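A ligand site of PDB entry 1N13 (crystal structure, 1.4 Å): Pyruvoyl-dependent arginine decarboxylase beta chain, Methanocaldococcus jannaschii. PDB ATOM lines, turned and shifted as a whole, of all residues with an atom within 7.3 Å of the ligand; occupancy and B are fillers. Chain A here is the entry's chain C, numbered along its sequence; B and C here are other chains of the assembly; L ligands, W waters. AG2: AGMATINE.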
ATOM      1  N   LEU A  31      -6.409 -15.738 -23.843  1.00  0.00           N
ATOM      2  CA  LEU A  31      -7.734 -15.188 -24.082  1.00  0.00           C
ATOM      3  C   LEU A  31      -7.700 -13.693 -24.399  1.00  0.00           C
ATOM      4  O   LEU A  31      -8.474 -13.213 -25.221  1.00  0.00           O
ATOM      5  CB  LEU A  31      -8.673 -15.491 -22.914  1.00  0.00           C
ATOM      6  CG  LEU A  31     -10.177 -15.313 -23.150  1.00  0.00           C
ATOM      7  CD1 LEU A  31     -10.600 -16.046 -24.423  1.00  0.00           C
ATOM      8  CD2 LEU A  31     -10.944 -15.844 -21.957  1.00  0.00           C
ATOM      9  N   ASN A  32      -6.795 -12.955 -23.748  1.00  0.00           N
ATOM     10  CA  ASN A  32      -6.671 -11.528 -24.005  1.00  0.00           C
ATOM     11  C   ASN A  32      -6.081 -11.276 -25.391  1.00  0.00           C
ATOM     12  O   ASN A  32      -6.442 -10.302 -26.044  1.00  0.00           O
ATOM     13  CB  ASN A  32      -5.819 -10.834 -22.931  1.00  0.00           C
ATOM     14  CG  ASN A  32      -6.561 -10.664 -21.618  1.00  0.00           C
ATOM     15  OD1 ASN A  32      -6.114 -11.115 -20.572  1.00  0.00           O
ATOM     16  ND2 ASN A  32      -7.708  -9.989 -21.674  1.00  0.00           N
ATOM     17  N   PHE A  34      -6.477 -13.375 -27.907  1.00  0.00           N
ATOM     18  CA  PHE A  34      -7.557 -13.792 -28.802  1.00  0.00           C
ATOM     19  C   PHE A  34      -8.524 -12.619 -28.947  1.00  0.00           C
ATOM     20  O   PHE A  34      -8.860 -12.211 -30.062  1.00  0.00           O
ATOM     21  CB  PHE A  34      -8.276 -15.021 -28.210  1.00  0.00           C
ATOM     22  CG  PHE A  34      -9.405 -15.545 -29.056  1.00  0.00           C
ATOM     23  CD1 PHE A  34      -9.154 -16.303 -30.194  1.00  0.00           C
ATOM     24  CD2 PHE A  34     -10.729 -15.298 -28.703  1.00  0.00           C
ATOM     25  CE1 PHE A  34     -10.202 -16.804 -30.968  1.00  0.00           C
ATOM     26  CE2 PHE A  34     -11.790 -15.798 -29.470  1.00  0.00           C
ATOM     27  CZ  PHE A  34     -11.526 -16.552 -30.603  1.00  0.00           C
ATOM     28  N   ASP A  35      -8.909 -12.032 -27.809  1.00  0.00           N
ATOM     29  CA  ASP A  35      -9.814 -10.888 -27.771  1.00  0.00           C
ATOM     30  C   ASP A  35      -9.217  -9.746 -28.602  1.00  0.00           C
ATOM     31  O   ASP A  35      -9.899  -9.129 -29.415  1.00  0.00           O
ATOM     32  CB  ASP A  35     -10.018 -10.438 -26.313  1.00  0.00           C
ATOM     33  CG  ASP A  35     -11.090  -9.369 -26.150  1.00  0.00           C
ATOM     34  OD1 ASP A  35     -12.092  -9.375 -26.899  1.00  0.00           O
ATOM     35  OD2 ASP A  35     -10.945  -8.521 -25.253  1.00  0.00           O
ATOM     36  N   GLY A  36      -7.914  -9.502 -28.424  1.00  0.00           N
ATOM     37  CA  GLY A  36      -7.257  -8.457 -29.180  1.00  0.00           C
ATOM     38  C   GLY A  36      -7.292  -8.707 -30.676  1.00  0.00           C
ATOM     39  O   GLY A  36      -7.423  -7.779 -31.463  1.00  0.00           O
ATOM     40  N   LEU A  38      -9.581 -10.446 -32.319  1.00  0.00           N
ATOM     41  CA  LEU A  38     -10.953 -10.224 -32.769  1.00  0.00           C
ATOM     42  C   LEU A  38     -11.187  -8.728 -32.924  1.00  0.00           C
ATOM     43  O   LEU A  38     -11.763  -8.280 -33.910  1.00  0.00           O
ATOM     44  CB  LEU A  38     -11.955 -10.819 -31.775  1.00  0.00           C
ATOM     45  CG  LEU A  38     -12.347 -12.286 -32.022  1.00  0.00           C
ATOM     46  CD1 LEU A  38     -11.139 -13.189 -31.984  1.00  0.00           C
ATOM     47  CD2 LEU A  38     -13.352 -12.702 -30.967  1.00  0.00           C
ATOM     48  N   LEU A  39     -10.704  -7.943 -31.958  1.00  0.00           N
ATOM     49  CA  LEU A  39     -10.844  -6.485 -32.020  1.00  0.00           C
ATOM     50  C   LEU A  39     -10.129  -5.942 -33.253  1.00  0.00           C
ATOM     51  O   LEU A  39     -10.661  -5.080 -33.960  1.00  0.00           O
ATOM     52  CB  LEU A  39     -10.250  -5.852 -30.754  1.00  0.00           C
ATOM     53  CG  LEU A  39     -11.123  -5.992 -29.513  1.00  0.00           C
ATOM     54  CD1 LEU A  39     -10.325  -5.670 -28.266  1.00  0.00           C
ATOM     55  CD2 LEU A  39     -12.342  -5.085 -29.632  1.00  0.00           C
ATOM     56  N   ILE A  43     -14.466  -7.661 -35.179  1.00  0.00           N
ATOM     57  CA  ILE A  43     -15.600  -8.370 -34.568  1.00  0.00           C
ATOM     58  C   ILE A  43     -15.374  -8.656 -33.084  1.00  0.00           C
ATOM     59  O   ILE A  43     -15.911  -9.632 -32.538  1.00  0.00           O
ATOM     60  CB  ILE A  43     -15.939  -9.690 -35.319  1.00  0.00           C
ATOM     61  CG1 ILE A  43     -14.703 -10.595 -35.438  1.00  0.00           C
ATOM     62  CG2 ILE A  43     -16.555  -9.393 -36.675  1.00  0.00           C
ATOM     63  CD1 ILE A  43     -15.006 -11.963 -36.022  1.00  0.00           C
ATOM     64  N   GLY A  44     -14.639  -7.769 -32.434  1.00  0.00           N
ATOM     65  CA  GLY A  44     -14.335  -7.949 -31.023  1.00  0.00           C
ATOM     66  C   GLY A  44     -15.484  -7.686 -30.064  1.00  0.00           C
ATOM     67  O   GLY A  44     -15.450  -8.142 -28.915  1.00  0.00           O
ATOM     68  N   ASN A  45     -16.526  -6.990 -30.529  1.00  0.00           N
ATOM     69  CA  ASN A  45     -17.636  -6.662 -29.648  1.00  0.00           C
ATOM     70  C   ASN A  45     -18.961  -7.377 -29.902  1.00  0.00           C
ATOM     71  O   ASN A  45     -20.029  -6.864 -29.552  1.00  0.00           O
ATOM     72  CB  ASN A  45     -17.808  -5.147 -29.574  1.00  0.00           C
ATOM     73  CG  ASN A  45     -16.584  -4.460 -28.979  1.00  0.00           C
ATOM     74  OD1 ASN A  45     -16.005  -4.966 -28.019  1.00  0.00           O
ATOM     75  ND2 ASN A  45     -16.185  -3.332 -29.557  1.00  0.00           N
ATOM     76  N   VAL A  46     -18.875  -8.536 -30.542  1.00  0.00           N
ATOM     77  CA  VAL A  46     -20.061  -9.360 -30.784  1.00  0.00           C
ATOM     78  C   VAL A  46     -19.725 -10.758 -30.294  1.00  0.00           C
ATOM     79  O   VAL A  46     -18.557 -11.069 -30.037  1.00  0.00           O
ATOM     80  CB  VAL A  46     -20.465  -9.428 -32.282  1.00  0.00           C
ATOM     81  CG1 VAL A  46     -20.864  -8.057 -32.792  1.00  0.00           C
ATOM     82  CG2 VAL A  46     -19.359 -10.013 -33.115  1.00  0.00           C
ATOM     83  N   ASN A  47     -20.749 -11.568 -30.102  1.00  0.00           N
ATOM     84  CA  ASN A  47     -20.564 -12.946 -29.644  1.00  0.00           C
ATOM     85  C   ASN A  47     -20.373 -13.868 -30.830  1.00  0.00           C
ATOM     86  O   ASN A  47     -21.178 -13.843 -31.759  1.00  0.00           O
ATOM     87  CB  ASN A  47     -21.778 -13.393 -28.834  1.00  0.00           C
ATOM     88  CG  ASN A  47     -21.811 -12.793 -27.467  1.00  0.00           C
ATOM     89  OD1 ASN A  47     -20.907 -13.030 -26.681  1.00  0.00           O
ATOM     90  ND2 ASN A  47     -22.823 -11.990 -27.178  1.00  0.00           N
ATOM     91  N   LEU A  48     -19.289 -14.636 -30.825  1.00  0.00           N
ATOM     92  CA  LEU A  48     -19.057 -15.565 -31.919  1.00  0.00           C
ATOM     93  C   LEU A  48     -19.667 -16.920 -31.576  1.00  0.00           C
ATOM     94  O   LEU A  48     -19.407 -17.475 -30.511  1.00  0.00           O
ATOM     95  CB  LEU A  48     -17.564 -15.741 -32.197  1.00  0.00           C
ATOM     96  CG  LEU A  48     -16.740 -14.507 -32.535  1.00  0.00           C
ATOM     97  CD1 LEU A  48     -15.376 -14.953 -33.040  1.00  0.00           C
ATOM     98  CD2 LEU A  48     -17.442 -13.678 -33.596  1.00  0.00           C
ATOM     99  C   PYR B   1     -18.345 -11.854 -24.292  1.00  0.00           C
ATOM    100  O   PYR B   1     -17.568 -11.058 -23.785  1.00  0.00           O
ATOM    101  CA  PYR B   1     -18.019 -13.235 -24.379  1.00  0.00           C
ATOM    102  O3  PYR B   1     -16.931 -13.581 -23.919  1.00  0.00           O
ATOM    103  CB  PYR B   1     -18.813 -14.360 -24.953  1.00  0.00           C
ATOM    104  N   ILE B   2     -19.524 -11.490 -24.804  1.00  0.00           N
ATOM    105  CA  ILE B   2     -19.980 -10.108 -24.779  1.00  0.00           C
ATOM    106  C   ILE B   2     -21.384  -9.920 -24.219  1.00  0.00           C
ATOM    107  O   ILE B   2     -22.329 -10.590 -24.645  1.00  0.00           O
ATOM    108  CB  ILE B   2     -19.954  -9.485 -26.213  1.00  0.00           C
ATOM    109  CG1 ILE B   2     -18.525  -9.429 -26.750  1.00  0.00           C
ATOM    110  CG2 ILE B   2     -20.569  -8.088 -26.201  1.00  0.00           C
ATOM    111  CD1 ILE B   2     -17.628  -8.444 -26.031  1.00  0.00           C
ATOM    112  N   ALA B  24     -21.232 -18.294 -22.095  1.00  0.00           N
ATOM    113  CA  ALA B  24     -19.781 -18.199 -22.090  1.00  0.00           C
ATOM    114  C   ALA B  24     -19.396 -19.033 -20.866  1.00  0.00           C
ATOM    115  O   ALA B  24     -19.999 -18.874 -19.801  1.00  0.00           O
ATOM    116  CB  ALA B  24     -19.327 -16.752 -21.901  1.00  0.00           C
ATOM    117  N   TYR B  25     -18.457 -19.939 -21.012  1.00  0.00           N
ATOM    118  CA  TYR B  25     -18.073 -20.750 -19.871  1.00  0.00           C
ATOM    119  C   TYR B  25     -16.639 -21.245 -19.907  1.00  0.00           C
ATOM    120  O   TYR B  25     -15.992 -21.245 -20.953  1.00  0.00           O
ATOM    121  CB  TYR B  25     -19.039 -21.940 -19.686  1.00  0.00           C
ATOM    122  CG  TYR B  25     -19.045 -22.975 -20.793  1.00  0.00           C
ATOM    123  CD1 TYR B  25     -18.066 -23.973 -20.861  1.00  0.00           C
ATOM    124  CD2 TYR B  25     -20.067 -22.994 -21.741  1.00  0.00           C
ATOM    125  CE1 TYR B  25     -18.111 -24.970 -21.839  1.00  0.00           C
ATOM    126  CE2 TYR B  25     -20.124 -23.989 -22.712  1.00  0.00           C
ATOM    127  CZ  TYR B  25     -19.146 -24.974 -22.755  1.00  0.00           C
ATOM    128  OH  TYR B  25     -19.206 -25.948 -23.721  1.00  0.00           O
ATOM    129  N   ILE B  41     -15.609 -16.899 -13.818  1.00  0.00           N
ATOM    130  CA  ILE B  41     -16.167 -16.038 -14.857  1.00  0.00           C
ATOM    131  C   ILE B  41     -16.228 -14.607 -14.319  1.00  0.00           C
ATOM    132  O   ILE B  41     -16.497 -14.392 -13.142  1.00  0.00           O
ATOM    133  CB  ILE B  41     -17.605 -16.478 -15.244  1.00  0.00           C
ATOM    134  CG1 ILE B  41     -17.565 -17.756 -16.080  1.00  0.00           C
ATOM    135  CG2 ILE B  41     -18.328 -15.384 -16.026  1.00  0.00           C
ATOM    136  CD1 ILE B  41     -17.314 -17.516 -17.568  1.00  0.00           C
ATOM    137  N   SER B  42     -15.979 -13.635 -15.190  1.00  0.00           N
ATOM    138  CA  SER B  42     -16.045 -12.235 -14.819  1.00  0.00           C
ATOM    139  C   SER B  42     -16.752 -11.467 -15.920  1.00  0.00           C
ATOM    140  O   SER B  42     -16.734 -11.884 -17.087  1.00  0.00           O
ATOM    141  CB  SER B  42     -14.648 -11.656 -14.597  1.00  0.00           C
ATOM    142  OG  SER B  42     -13.881 -11.743 -15.777  1.00  0.00           O
ATOM    143  N   LEU B  54     -17.825  -7.017 -21.039  1.00  0.00           N
ATOM    144  CA  LEU B  54     -16.897  -8.052 -21.492  1.00  0.00           C
ATOM    145  C   LEU B  54     -16.879  -9.230 -20.532  1.00  0.00           C
ATOM    146  O   LEU B  54     -16.601  -9.070 -19.345  1.00  0.00           O
ATOM    147  CB  LEU B  54     -15.488  -7.477 -21.623  1.00  0.00           C
ATOM    148  CG  LEU B  54     -14.391  -8.452 -22.060  1.00  0.00           C
ATOM    149  CD1 LEU B  54     -14.645  -8.984 -23.465  1.00  0.00           C
ATOM    150  CD2 LEU B  54     -13.047  -7.732 -21.997  1.00  0.00           C
ATOM    151  N   ILE B  55     -17.145 -10.413 -21.072  1.00  0.00           N
ATOM    152  CA  ILE B  55     -17.162 -11.638 -20.271  1.00  0.00           C
ATOM    153  C   ILE B  55     -15.857 -12.406 -20.501  1.00  0.00           C
ATOM    154  O   ILE B  55     -15.442 -12.621 -21.633  1.00  0.00           O
ATOM    155  CB  ILE B  55     -18.350 -12.543 -20.647  1.00  0.00           C
ATOM    156  CG1 ILE B  55     -19.666 -11.771 -20.498  1.00  0.00           C
ATOM    157  CG2 ILE B  55     -18.375 -13.781 -19.754  1.00  0.00           C
ATOM    158  CD1 ILE B  55     -20.853 -12.487 -21.109  1.00  0.00           C
ATOM    159  N   MET B  56     -15.222 -12.784 -19.405  1.00  0.00           N
ATOM    160  CA  MET B  56     -13.980 -13.537 -19.456  1.00  0.00           C
ATOM    161  C   MET B  56     -14.135 -14.804 -18.633  1.00  0.00           C
ATOM    162  O   MET B  56     -14.876 -14.825 -17.651  1.00  0.00           O
ATOM    163  CB  MET B  56     -12.824 -12.698 -18.900  1.00  0.00           C
ATOM    164  CG  MET B  56     -12.282 -11.666 -19.883  1.00  0.00           C
ATOM    165  SD  MET B  56     -11.323 -12.473 -21.182  1.00  0.00           S
ATOM    166  CE  MET B  56     -11.021 -11.113 -22.321  1.00  0.00           C
ATOM    167  N   GLU B  57     -13.485 -15.881 -19.085  1.00  0.00           N
ATOM    168  CA  GLU B  57     -13.531 -17.156 -18.387  1.00  0.00           C
ATOM    169  C   GLU B  57     -12.119 -17.645 -18.119  1.00  0.00           C
ATOM    170  O   GLU B  57     -11.192 -17.352 -18.873  1.00  0.00           O
ATOM    171  CB  GLU B  57     -14.313 -18.212 -19.192  1.00  0.00           C
ATOM    172  CG  GLU B  57     -13.747 -18.552 -20.556  1.00  0.00           C
ATOM    173  CD  GLU B  57     -14.368 -17.727 -21.674  1.00  0.00           C
ATOM    174  OE1 GLU B  57     -14.923 -18.312 -22.624  1.00  0.00           O
ATOM    175  OE2 GLU B  57     -14.295 -16.491 -21.595  1.00  0.00           O
ATOM    176  N   ARG B  82      -9.542  -1.882 -25.108  1.00  0.00           N
ATOM    177  CA  ARG B  82     -10.573  -1.138 -25.833  1.00  0.00           C
ATOM    178  C   ARG B  82     -10.529   0.356 -25.503  1.00  0.00           C
ATOM    179  O   ARG B  82     -11.110   1.180 -26.217  1.00  0.00           O
ATOM    180  CB  ARG B  82     -11.968  -1.682 -25.488  1.00  0.00           C
ATOM    181  CG  ARG B  82     -12.263  -3.047 -26.058  1.00  0.00           C
ATOM    182  CD  ARG B  82     -13.545  -3.613 -25.453  1.00  0.00           C
ATOM    183  NE  ARG B  82     -13.983  -4.830 -26.125  1.00  0.00           N
ATOM    184  CZ  ARG B  82     -13.389  -6.017 -25.997  1.00  0.00           C
ATOM    185  NH1 ARG B  82     -12.329  -6.159 -25.212  1.00  0.00           N
ATOM    186  NH2 ARG B  82     -13.844  -7.060 -26.692  1.00  0.00           N
ATOM    187  N   ILE C  51     -20.374 -19.485 -26.451  1.00  0.00           N
ATOM    188  CA  ILE C  51     -20.027 -18.274 -27.160  1.00  0.00           C
ATOM    189  C   ILE C  51     -18.542 -18.008 -26.993  1.00  0.00           C
ATOM    190  O   ILE C  51     -17.951 -18.345 -25.958  1.00  0.00           O
ATOM    191  CB  ILE C  51     -20.876 -17.063 -26.703  1.00  0.00           C
ATOM    192  CG1 ILE C  51     -20.783 -16.873 -25.191  1.00  0.00           C
ATOM    193  CG2 ILE C  51     -22.331 -17.267 -27.096  1.00  0.00           C
ATOM    194  CD1 ILE C  51     -21.744 -15.815 -24.656  1.00  0.00           C
ATOM    195  N   SER C  52     -17.925 -17.468 -28.031  1.00  0.00           N
ATOM    196  CA  SER C  52     -16.496 -17.176 -27.990  1.00  0.00           C
ATOM    197  C   SER C  52     -16.167 -15.758 -28.447  1.00  0.00           C
ATOM    198  O   SER C  52     -14.968 -15.410 -28.380  1.00  0.00           O
ATOM    199  CB  SER C  52     -15.723 -18.186 -28.841  1.00  0.00           C
ATOM    200  OG  SER C  52     -16.238 -18.245 -30.158  1.00  0.00           O
ATOM    201  OXT SER C  52     -17.084 -15.002 -28.857  1.00  0.00           O
HETATM  202  N   AG2 L   1     -14.763 -14.777 -23.445  1.00  0.00           N
HETATM  203  CA  AG2 L   1     -13.730 -14.165 -24.312  1.00  0.00           C
HETATM  204  CB  AG2 L   1     -14.152 -12.761 -24.722  1.00  0.00           C
HETATM  205  CG  AG2 L   1     -13.170 -12.059 -25.627  1.00  0.00           C
HETATM  206  CD  AG2 L   1     -13.040 -12.757 -26.974  1.00  0.00           C
HETATM  207  NE  AG2 L   1     -14.327 -12.862 -27.662  1.00  0.00           N
HETATM  208  CZ  AG2 L   1     -15.024 -11.834 -28.142  1.00  0.00           C
HETATM  209  NH1 AG2 L   1     -14.576 -10.587 -28.013  1.00  0.00           N
HETATM  210  NH2 AG2 L   1     -16.185 -12.055 -28.736  1.00  0.00           N
HETATM  211  O   HOH W   1     -16.061 -16.901 -24.755  1.00  0.00           O
HETATM  212  O   HOH W   2     -13.592 -16.844 -26.417  1.00  0.00           O
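O of PYR 1 of chain B lies within hydrogen-bond range of N of Ile 55 of chain B, at 2.8 Å. The backbone carbonyl oxygen (O) of Leu 48 is in hydrogen-bond range of the backbone NH (N) of Ser 52 of chain C. The backbone carbonyl oxygen of Leu 38 sits at hydrogen-bond distance from the backbone NH of Gly 44 (3.3 Å). O of Gly 44 sits at hydrogen-bond distance from NH2 of Arg 82 of chain B. The side-chain carboxylate (OD2) of Asp 35 is in salt-bridge range of the guanidinium group (NH1) of Arg 82 of chain B (2.7 Å). N of Ile 43 sits at hydrogen-bond distance from O of Leu 38, at 3.0 Å. NE of Arg 82 of chain B lies within hydrogen-bond range of OD1 of Asn 45 (2.8 Å).
Water W1 lies within hydrogen-bond range of the backbone carbonyl oxygen (O) of Ile 51 of chain C (2.7 Å), the side-chain carboxylate (OE1) of Glu 57 of chain B (2.8 Å) and a nitrogen (N) of the ligand (2.8 Å).
Residues that only touch the ligand: Leu 38, Leu 31, Arg 82 of chain B and Phe 34. Hydrophobic or aromatic side chains that line the ligand: Leu 31, Phe 34 and Leu 38.
N of the ligand is in hydrogen-bond range of O3 of PYR 1 of chain B, 2.5 Å away. A nitrogen (N) of the ligand lies within salt-bridge range of the side-chain carboxylate (OE2) of Glu 57 of chain B (2.6 Å). O of Ser 52 of chain C lies within salt-bridge range of NE of the ligand, 2.7 Å away. The backbone carbonyl oxygen (O) of Gly 44 sits at hydrogen-bond distance from a nitrogen (NH1) of the ligand (2.7 Å). A nitrogen (NH2) of the ligand sits at hydrogen-bond distance from the backbone carbonyl oxygen (O) of Val 46 (2.9 Å). The backbone carbonyl oxygen of Ile 55 of chain B sits at hydrogen-bond distance from a nitrogen (N) of the ligand. NH1 of the ligand lies within salt-bridge range of OD1 of Asp 35 (3.0 Å).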
